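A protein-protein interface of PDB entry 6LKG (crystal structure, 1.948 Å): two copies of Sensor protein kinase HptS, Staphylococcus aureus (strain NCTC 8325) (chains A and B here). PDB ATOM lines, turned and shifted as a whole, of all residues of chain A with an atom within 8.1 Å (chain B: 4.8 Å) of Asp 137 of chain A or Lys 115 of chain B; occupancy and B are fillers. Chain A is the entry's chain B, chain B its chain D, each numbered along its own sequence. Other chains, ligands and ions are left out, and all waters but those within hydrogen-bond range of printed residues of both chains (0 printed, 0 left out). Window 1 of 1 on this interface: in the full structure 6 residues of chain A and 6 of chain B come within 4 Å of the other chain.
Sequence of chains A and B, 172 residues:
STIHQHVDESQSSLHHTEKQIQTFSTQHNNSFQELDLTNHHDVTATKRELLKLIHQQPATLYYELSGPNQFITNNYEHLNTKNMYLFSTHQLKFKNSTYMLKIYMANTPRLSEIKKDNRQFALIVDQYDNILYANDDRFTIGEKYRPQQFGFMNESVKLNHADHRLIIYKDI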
ATOM      1  N   LYS A 115     -14.840  43.262  -8.775  1.00  0.00           N
ATOM      2  CA  LYS A 115     -15.544  42.043  -8.397  1.00  0.00           C
ATOM      3  C   LYS A 115     -17.033  42.313  -8.211  1.00  0.00           C
ATOM      4  O   LYS A 115     -17.876  41.540  -8.681  1.00  0.00           O
ATOM      5  CB  LYS A 115     -14.937  41.463  -7.117  1.00  0.00           C
ATOM      6  CG  LYS A 115     -15.713  40.298  -6.525  1.00  0.00           C
ATOM      7  CD  LYS A 115     -15.077  39.813  -5.230  1.00  0.00           C
ATOM      8  CE  LYS A 115     -15.881  38.681  -4.607  1.00  0.00           C
ATOM      9  NZ  LYS A 115     -15.262  38.178  -3.349  1.00  0.00           N
ATOM     10  N   PHE A 121     -12.879  38.552 -11.062  1.00  0.00           N
ATOM     11  CA  PHE A 121     -12.144  38.079  -9.899  1.00  0.00           C
ATOM     12  C   PHE A 121     -10.642  38.132 -10.156  1.00  0.00           C
ATOM     13  O   PHE A 121     -10.181  38.301 -11.286  1.00  0.00           O
ATOM     14  CB  PHE A 121     -12.578  36.658  -9.533  1.00  0.00           C
ATOM     15  CG  PHE A 121     -14.056  36.515  -9.322  1.00  0.00           C
ATOM     16  CD1 PHE A 121     -14.631  36.857  -8.108  1.00  0.00           C
ATOM     17  CD2 PHE A 121     -14.874  36.047 -10.336  1.00  0.00           C
ATOM     18  CE1 PHE A 121     -15.994  36.729  -7.910  1.00  0.00           C
ATOM     19  CE2 PHE A 121     -16.236  35.918 -10.145  1.00  0.00           C
ATOM     20  CZ  PHE A 121     -16.797  36.259  -8.931  1.00  0.00           C
ATOM     21  N   ALA A 134      -6.560  35.083  -3.749  1.00  0.00           N
ATOM     22  CA  ALA A 134      -7.811  34.855  -4.452  1.00  0.00           C
ATOM     23  C   ALA A 134      -8.913  35.613  -3.729  1.00  0.00           C
ATOM     24  O   ALA A 134      -8.897  35.713  -2.500  1.00  0.00           O
ATOM     25  CB  ALA A 134      -8.149  33.361  -4.524  1.00  0.00           C
ATOM     26  N   ASN A 135      -9.861  36.152  -4.498  1.00  0.00           N
ATOM     27  CA  ASN A 135     -11.078  36.720  -3.927  1.00  0.00           C
ATOM     28  C   ASN A 135     -12.311  35.985  -4.436  1.00  0.00           C
ATOM     29  O   ASN A 135     -13.413  36.543  -4.443  1.00  0.00           O
ATOM     30  CB  ASN A 135     -11.177  38.222  -4.214  1.00  0.00           C
ATOM     31  CG  ASN A 135     -11.131  38.551  -5.698  1.00  0.00           C
ATOM     32  OD1 ASN A 135     -11.134  37.664  -6.552  1.00  0.00           O
ATOM     33  ND2 ASN A 135     -11.092  39.843  -6.010  1.00  0.00           N
ATOM     34  N   ASP A 136     -12.131  34.738  -4.864  1.00  0.00           N
ATOM     35  CA  ASP A 136     -13.200  33.857  -5.308  1.00  0.00           C
ATOM     36  C   ASP A 136     -13.111  32.581  -4.484  1.00  0.00           C
ATOM     37  O   ASP A 136     -12.046  31.956  -4.420  1.00  0.00           O
ATOM     38  CB  ASP A 136     -13.068  33.558  -6.806  1.00  0.00           C
ATOM     39  CG  ASP A 136     -14.204  32.701  -7.350  1.00  0.00           C
ATOM     40  OD1 ASP A 136     -15.114  32.327  -6.583  1.00  0.00           O
ATOM     41  OD2 ASP A 136     -14.178  32.403  -8.563  1.00  0.00           O
ATOM     42  N   ASP A 137     -14.226  32.192  -3.862  1.00  0.00           N
ATOM     43  CA  ASP A 137     -14.195  31.107  -2.885  1.00  0.00           C
ATOM     44  C   ASP A 137     -13.921  29.741  -3.502  1.00  0.00           C
ATOM     45  O   ASP A 137     -13.652  28.794  -2.755  1.00  0.00           O
ATOM     46  CB  ASP A 137     -15.502  31.069  -2.084  1.00  0.00           C
ATOM     47  CG  ASP A 137     -16.732  30.879  -2.955  1.00  0.00           C
ATOM     48  OD1 ASP A 137     -16.597  30.515  -4.143  1.00  0.00           O
ATOM     49  OD2 ASP A 137     -17.848  31.092  -2.438  1.00  0.00           O
ATOM     50  N   ARG A 138     -13.984  29.603  -4.825  1.00  0.00           N
ATOM     51  CA  ARG A 138     -13.645  28.325  -5.437  1.00  0.00           C
ATOM     52  C   ARG A 138     -12.142  28.096  -5.515  1.00  0.00           C
ATOM     53  O   ARG A 138     -11.716  27.029  -5.969  1.00  0.00           O
ATOM     54  CB  ARG A 138     -14.247  28.213  -6.840  1.00  0.00           C
ATOM     55  CG  ARG A 138     -13.718  29.219  -7.846  1.00  0.00           C
ATOM     56  CD  ARG A 138     -14.442  29.078  -9.179  1.00  0.00           C
ATOM     57  NE  ARG A 138     -14.614  30.357  -9.862  1.00  0.00           N
ATOM     58  CZ  ARG A 138     -15.276  30.506 -11.004  1.00  0.00           C
ATOM     59  NH1 ARG A 138     -15.829  29.455 -11.593  1.00  0.00           N
ATOM     60  NH2 ARG A 138     -15.386  31.705 -11.558  1.00  0.00           N
ATOM     61  N   PHE A 139     -11.335  29.065  -5.088  1.00  0.00           N
ATOM     62  CA  PHE A 139      -9.889  28.928  -5.045  1.00  0.00           C
ATOM     63  C   PHE A 139      -9.406  29.164  -3.622  1.00  0.00           C
ATOM     64  O   PHE A 139      -9.848  30.101  -2.951  1.00  0.00           O
ATOM     65  CB  PHE A 139      -9.208  29.908  -6.005  1.00  0.00           C
ATOM     66  CG  PHE A 139      -9.501  29.637  -7.451  1.00  0.00           C
ATOM     67  CD1 PHE A 139      -9.021  28.490  -8.064  1.00  0.00           C
ATOM     68  CD2 PHE A 139     -10.252  30.529  -8.199  1.00  0.00           C
ATOM     69  CE1 PHE A 139      -9.289  28.235  -9.393  1.00  0.00           C
ATOM     70  CE2 PHE A 139     -10.522  30.280  -9.532  1.00  0.00           C
ATOM     71  CZ  PHE A 139     -10.040  29.131 -10.130  1.00  0.00           C
ATOM     72  N   THR A 140      -8.496  28.309  -3.166  1.00  0.00           N
ATOM     73  CA  THR A 140      -7.965  28.370  -1.813  1.00  0.00           C
ATOM     74  C   THR A 140      -6.475  28.665  -1.880  1.00  0.00           C
ATOM     75  O   THR A 140      -5.738  27.987  -2.604  1.00  0.00           O
ATOM     76  CB  THR A 140      -8.214  27.059  -1.061  1.00  0.00           C
ATOM     77  OG1 THR A 140      -9.625  26.829  -0.954  1.00  0.00           O
ATOM     78  CG2 THR A 140      -7.606  27.114   0.331  1.00  0.00           C
ATOM     79  N   ILE A 141      -6.042  29.681  -1.129  1.00  0.00           N
ATOM     80  CA  ILE A 141      -4.623  30.003  -1.057  1.00  0.00           C
ATOM     81  C   ILE A 141      -3.862  28.797  -0.530  1.00  0.00           C
ATOM     82  O   ILE A 141      -4.228  28.208   0.494  1.00  0.00           O
ATOM     83  CB  ILE A 141      -4.401  31.241  -0.174  1.00  0.00           C
ATOM     84  CG1 ILE A 141      -4.944  32.493  -0.866  1.00  0.00           C
ATOM     85  CG2 ILE A 141      -2.925  31.409   0.162  1.00  0.00           C
ATOM     86  CD1 ILE A 141      -4.803  33.751  -0.043  1.00  0.00           C
ATOM     87  N   GLU A 143      -3.350  26.049  -2.540  1.00  0.00           N
ATOM     88  CA  GLU A 143      -3.625  24.974  -3.475  1.00  0.00           C
ATOM     89  C   GLU A 143      -3.139  25.366  -4.866  1.00  0.00           C
ATOM     90  O   GLU A 143      -2.630  26.467  -5.093  1.00  0.00           O
ATOM     91  CB  GLU A 143      -5.114  24.630  -3.480  1.00  0.00           C
ATOM     92  CG  GLU A 143      -5.640  24.178  -2.127  1.00  0.00           C
ATOM     93  CD  GLU A 143      -7.086  23.726  -2.176  1.00  0.00           C
ATOM     94  OE1 GLU A 143      -7.739  23.915  -3.224  1.00  0.00           O
ATOM     95  OE2 GLU A 143      -7.571  23.181  -1.163  1.00  0.00           O
ATOM     96  N   TYR A 169     -10.090  37.612 -14.105  1.00  0.00           N
ATOM     97  CA  TYR A 169     -10.903  36.749 -14.947  1.00  0.00           C
ATOM     98  C   TYR A 169     -12.383  36.998 -14.701  1.00  0.00           C
ATOM     99  O   TYR A 169     -12.783  37.566 -13.681  1.00  0.00           O
ATOM    100  CB  TYR A 169     -10.568  35.270 -14.723  1.00  0.00           C
ATOM    101  CG  TYR A 169     -10.830  34.765 -13.323  1.00  0.00           C
ATOM    102  CD1 TYR A 169      -9.898  34.950 -12.311  1.00  0.00           C
ATOM    103  CD2 TYR A 169     -12.008  34.095 -13.016  1.00  0.00           C
ATOM    104  CE1 TYR A 169     -10.131  34.488 -11.033  1.00  0.00           C
ATOM    105  CE2 TYR A 169     -12.251  33.629 -11.739  1.00  0.00           C
ATOM    106  CZ  TYR A 169     -11.307  33.826 -10.753  1.00  0.00           C
ATOM    107  OH  TYR A 169     -11.540  33.368  -9.480  1.00  0.00           O
ATOM    108  N   LEU B 111     -26.937  21.794  -4.185  1.00  0.00           N
ATOM    109  CA  LEU B 111     -26.580  23.208  -4.238  1.00  0.00           C
ATOM    110  C   LEU B 111     -25.079  23.397  -4.425  1.00  0.00           C
ATOM    111  O   LEU B 111     -24.648  24.314  -5.133  1.00  0.00           O
ATOM    112  CB  LEU B 111     -27.061  23.911  -2.972  1.00  0.00           C
ATOM    113  CG  LEU B 111     -28.582  23.996  -2.830  1.00  0.00           C
ATOM    114  CD1 LEU B 111     -28.963  24.737  -1.557  1.00  0.00           C
ATOM    115  CD2 LEU B 111     -29.213  24.644  -4.055  1.00  0.00           C
ATOM    116  N   SER B 112     -24.269  22.543  -3.794  1.00  0.00           N
ATOM    117  CA  SER B 112     -22.820  22.668  -3.912  1.00  0.00           C
ATOM    118  C   SER B 112     -22.342  22.370  -5.327  1.00  0.00           C
ATOM    119  O   SER B 112     -21.417  23.024  -5.823  1.00  0.00           O
ATOM    120  CB  SER B 112     -22.128  21.738  -2.915  1.00  0.00           C
ATOM    121  OG  SER B 112     -22.375  22.142  -1.580  1.00  0.00           O
ATOM    122  N   GLU B 113     -22.955  21.390  -5.994  1.00  0.00           N
ATOM    123  CA  GLU B 113     -22.496  21.027  -7.330  1.00  0.00           C
ATOM    124  C   GLU B 113     -22.841  22.102  -8.353  1.00  0.00           C
ATOM    125  O   GLU B 113     -22.004  22.452  -9.193  1.00  0.00           O
ATOM    126  CB  GLU B 113     -23.072  19.673  -7.745  1.00  0.00           C
ATOM    127  CG  GLU B 113     -22.965  19.402  -9.233  1.00  0.00           C
ATOM    128  CD  GLU B 113     -22.904  17.926  -9.563  1.00  0.00           C
ATOM    129  OE1 GLU B 113     -23.917  17.389 -10.052  1.00  0.00           O
ATOM    130  OE2 GLU B 113     -21.840  17.310  -9.347  1.00  0.00           O
ATOM    131  N   ILE B 114     -24.066  22.631  -8.313  1.00  0.00           N
ATOM    132  CA  ILE B 114     -24.445  23.644  -9.296  1.00  0.00           C
ATOM    133  C   ILE B 114     -23.678  24.942  -9.072  1.00  0.00           C
ATOM    134  O   ILE B 114     -23.479  25.720 -10.013  1.00  0.00           O
ATOM    135  CB  ILE B 114     -25.968  23.874  -9.280  1.00  0.00           C
ATOM    136  CG1 ILE B 114     -26.404  24.536  -7.972  1.00  0.00           C
ATOM    137  CG2 ILE B 114     -26.704  22.558  -9.482  1.00  0.00           C
ATOM    138  CD1 ILE B 114     -27.842  25.001  -7.984  1.00  0.00           C
ATOM    139  N   LYS B 115     -23.230  25.203  -7.840  1.00  0.00           N
ATOM    140  CA  LYS B 115     -22.355  26.350  -7.618  1.00  0.00           C
ATOM    141  C   LYS B 115     -20.998  26.136  -8.273  1.00  0.00           C
ATOM    142  O   LYS B 115     -20.459  27.046  -8.915  1.00  0.00           O
ATOM    143  CB  LYS B 115     -22.187  26.616  -6.122  1.00  0.00           C
ATOM    144  CG  LYS B 115     -21.142  27.685  -5.813  1.00  0.00           C
ATOM    145  CD  LYS B 115     -20.959  27.906  -4.318  1.00  0.00           C
ATOM    146  CE  LYS B 115     -19.877  28.944  -4.054  1.00  0.00           C
ATOM    147  NZ  LYS B 115     -19.675  29.213  -2.603  1.00  0.00           N
ATOM    148  N   LYS B 116     -20.435  24.936  -8.129  1.00  0.00           N
ATOM    149  CA  LYS B 116     -19.119  24.658  -8.694  1.00  0.00           C
ATOM    150  C   LYS B 116     -19.180  24.557 -10.214  1.00  0.00           C
ATOM    151  O   LYS B 116     -18.363  25.160 -10.918  1.00  0.00           O
ATOM    152  CB  LYS B 116     -18.552  23.374  -8.086  1.00  0.00           C
ATOM    153  CG  LYS B 116     -17.280  22.880  -8.754  1.00  0.00           C
ATOM    154  CD  LYS B 116     -17.038  21.409  -8.457  1.00  0.00           C
ATOM    155  CE  LYS B 116     -15.829  20.889  -9.217  1.00  0.00           C
ATOM    156  NZ  LYS B 116     -14.558  21.440  -8.667  1.00  0.00           N
ATOM    157  N   ASP B 117     -20.143  23.798 -10.738  1.00  0.00           N
ATOM    158  CA  ASP B 117     -20.184  23.493 -12.163  1.00  0.00           C
ATOM    159  C   ASP B 117     -20.899  24.552 -12.995  1.00  0.00           C
ATOM    160  O   ASP B 117     -20.530  24.762 -14.157  1.00  0.00           O
ATOM    161  CB  ASP B 117     -20.864  22.140 -12.394  1.00  0.00           C
ATOM    162  CG  ASP B 117     -20.080  20.983 -11.802  1.00  0.00           C
ATOM    163  OD1 ASP B 117     -18.862  21.135 -11.580  1.00  0.00           O
ATOM    164  OD2 ASP B 117     -20.686  19.917 -11.561  1.00  0.00           O
ATOM    165  N   ASN B 118     -21.908  25.226 -12.443  1.00  0.00           N
ATOM    166  CA  ASN B 118     -22.719  26.161 -13.213  1.00  0.00           C
ATOM    167  C   ASN B 118     -22.651  27.597 -12.712  1.00  0.00           C
ATOM    168  O   ASN B 118     -23.259  28.478 -13.333  1.00  0.00           O
ATOM    169  CB  ASN B 118     -24.188  25.711 -13.221  1.00  0.00           C
ATOM    170  CG  ASN B 118     -24.353  24.256 -13.609  1.00  0.00           C
ATOM    171  OD1 ASN B 118     -24.792  23.434 -12.804  1.00  0.00           O
ATOM    172  ND2 ASN B 118     -24.009  23.931 -14.850  1.00  0.00           N
ATOM    173  N   ARG B 119     -21.930  27.859 -11.622  1.00  0.00           N
ATOM    174  CA  ARG B 119     -21.903  29.178 -10.985  1.00  0.00           C
ATOM    175  C   ARG B 119     -23.316  29.654 -10.660  1.00  0.00           C
ATOM    176  O   ARG B 119     -23.645  30.836 -10.780  1.00  0.00           O
ATOM    177  CB  ARG B 119     -21.161  30.206 -11.843  1.00  0.00           C
ATOM    178  CG  ARG B 119     -19.712  29.843 -12.145  1.00  0.00           C
ATOM    179  CD  ARG B 119     -18.983  29.342 -10.904  1.00  0.00           C
ATOM    180  NE  ARG B 119     -18.685  30.400  -9.943  1.00  0.00           N
ATOM    181  CZ  ARG B 119     -18.234  30.176  -8.712  1.00  0.00           C
ATOM    182  NH1 ARG B 119     -18.034  28.932  -8.294  1.00  0.00           N
ATOM    183  NH2 ARG B 119     -17.985  31.193  -7.898  1.00  0.00           N
ATOM    184  N   GLN B 120     -24.168  28.714 -10.256  1.00  0.00           N
ATOM    185  CA  GLN B 120     -25.518  29.011  -9.804  1.00  0.00           C
ATOM    186  C   GLN B 120     -25.527  28.976  -8.281  1.00  0.00           C
ATOM    187  O   GLN B 120     -25.245  27.934  -7.679  1.00  0.00           O
ATOM    188  CB  GLN B 120     -26.527  28.012 -10.373  1.00  0.00           C
ATOM    189  CG  GLN B 120     -26.722  28.108 -11.879  1.00  0.00           C
ATOM    190  CD  GLN B 120     -27.606  27.001 -12.427  1.00  0.00           C
ATOM    191  OE1 GLN B 120     -28.334  26.342 -11.682  1.00  0.00           O
ATOM    192  NE2 GLN B 120     -27.545  26.790 -13.737  1.00  0.00           N
ATOM    193  N   PHE B 121     -25.841  30.111  -7.666  1.00  0.00           N
ATOM    194  CA  PHE B 121     -25.834  30.245  -6.218  1.00  0.00           C
ATOM    195  C   PHE B 121     -27.243  30.072  -5.664  1.00  0.00           C
ATOM    196  O   PHE B 121     -28.233  30.071  -6.398  1.00  0.00           O
ATOM    197  CB  PHE B 121     -25.259  31.604  -5.805  1.00  0.00           C
ATOM    198  CG  PHE B 121     -23.901  31.886  -6.383  1.00  0.00           C
ATOM    199  CD1 PHE B 121     -22.761  31.365  -5.793  1.00  0.00           C
ATOM    200  CD2 PHE B 121     -23.764  32.675  -7.514  1.00  0.00           C
ATOM    201  CE1 PHE B 121     -21.508  31.623  -6.323  1.00  0.00           C
ATOM    202  CE2 PHE B 121     -22.516  32.938  -8.049  1.00  0.00           C
ATOM    203  CZ  PHE B 121     -21.386  32.410  -7.454  1.00  0.00           C
ATOM    204  N   ASN B 135     -24.814  30.792  -0.141  1.00  0.00           N
ATOM    205  CA  ASN B 135     -23.494  30.264  -0.473  1.00  0.00           C
ATOM    206  C   ASN B 135     -22.740  31.217  -1.398  1.00  0.00           C
ATOM    207  O   ASN B 135     -21.859  30.802  -2.153  1.00  0.00           O
ATOM    208  CB  ASN B 135     -23.595  28.864  -1.079  1.00  0.00           C
ATOM    209  CG  ASN B 135     -24.479  28.811  -2.312  1.00  0.00           C
ATOM    210  OD1 ASN B 135     -24.944  29.835  -2.811  1.00  0.00           O
ATOM    211  ND2 ASN B 135     -24.715  27.600  -2.811  1.00  0.00           N
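Positions printed for both chains: 115, 121 and 135.
Of the 3 pairs that touch across the chains among the printed residues, none has its exchanged pair printed and touching as well.
Of the 12 printed residues of chain B, 2 touch a printed residue of chain A.
Printed residues of chain B that touch a printed residue of chain A: Lys 115 and Arg 119.
Among the printed residues, Asp or Glu carboxylates within 4 Å of a Lys or Arg side-chain nitrogen of the other chain: Asp 136 of chain A with Arg 119 of chain B (3.4 Å) and Asp 137 of chain A with Lys 115 of chain B (2.6 Å).
The guanidinium group of Arg 119 of chain B lies within salt-bridge range of the side-chain carboxylate of Asp 136 of chain A.
NZ of Lys 115 of chain B lies within salt-bridge range of OD2 of Asp 137 of chain A, 2.6 Å away.
The guanidinium group (NH1) of Arg 138 of chain A sits close to the guanidinium group (NE) of Arg 119 of chain B (3.4 Å).
The side-chain carboxylate (OD2) of Asp 136 of chain A is in salt-bridge range of the guanidinium group (NE) of Arg 138 of chain A (2.5 Å).
The side-chain hydroxyl (OH) of Tyr 169 of chain A is in hydrogen-bond range of the side-chain carboxylate (OD2) of Asp 136 of chain A, 3.0 Å away.
The backbone carbonyl oxygen (O) of Ile 114 of chain B sits at hydrogen-bond distance from the backbone NH (N) of Arg 119 of chain B.
The backbone carbonyl oxygen of Lys 115 of chain B is in hydrogen-bond range of the guanidinium group of Arg 119 of chain B (3.1 Å).
The backbone NH (N) of Lys 115 of chain B sits close to the backbone carbonyl oxygen (O) of Gln 120 of chain B (3.4 Å).
The side-chain amino group (NZ) of Lys 115 of chain B is in hydrogen-bond range of the backbone carbonyl oxygen (O) of Asn 135 of chain B (2.7 Å).
Of the printed residues of chain B, Asp 136 of chain A touches Arg 119 (3.4 Å).
Asp 137 of chain A touches one residue of chain B.
Of the printed residues of chain B, Arg 138 of chain A touches Arg 119.
Ser 112 of chain B touches none of the printed residues of chain A.
Lys 115 of chain B touches just one residue of chain A: Asp 137.
Printed residues of chain A within 4 Å of Arg 119 of chain B: Asp 136 and Arg 138.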
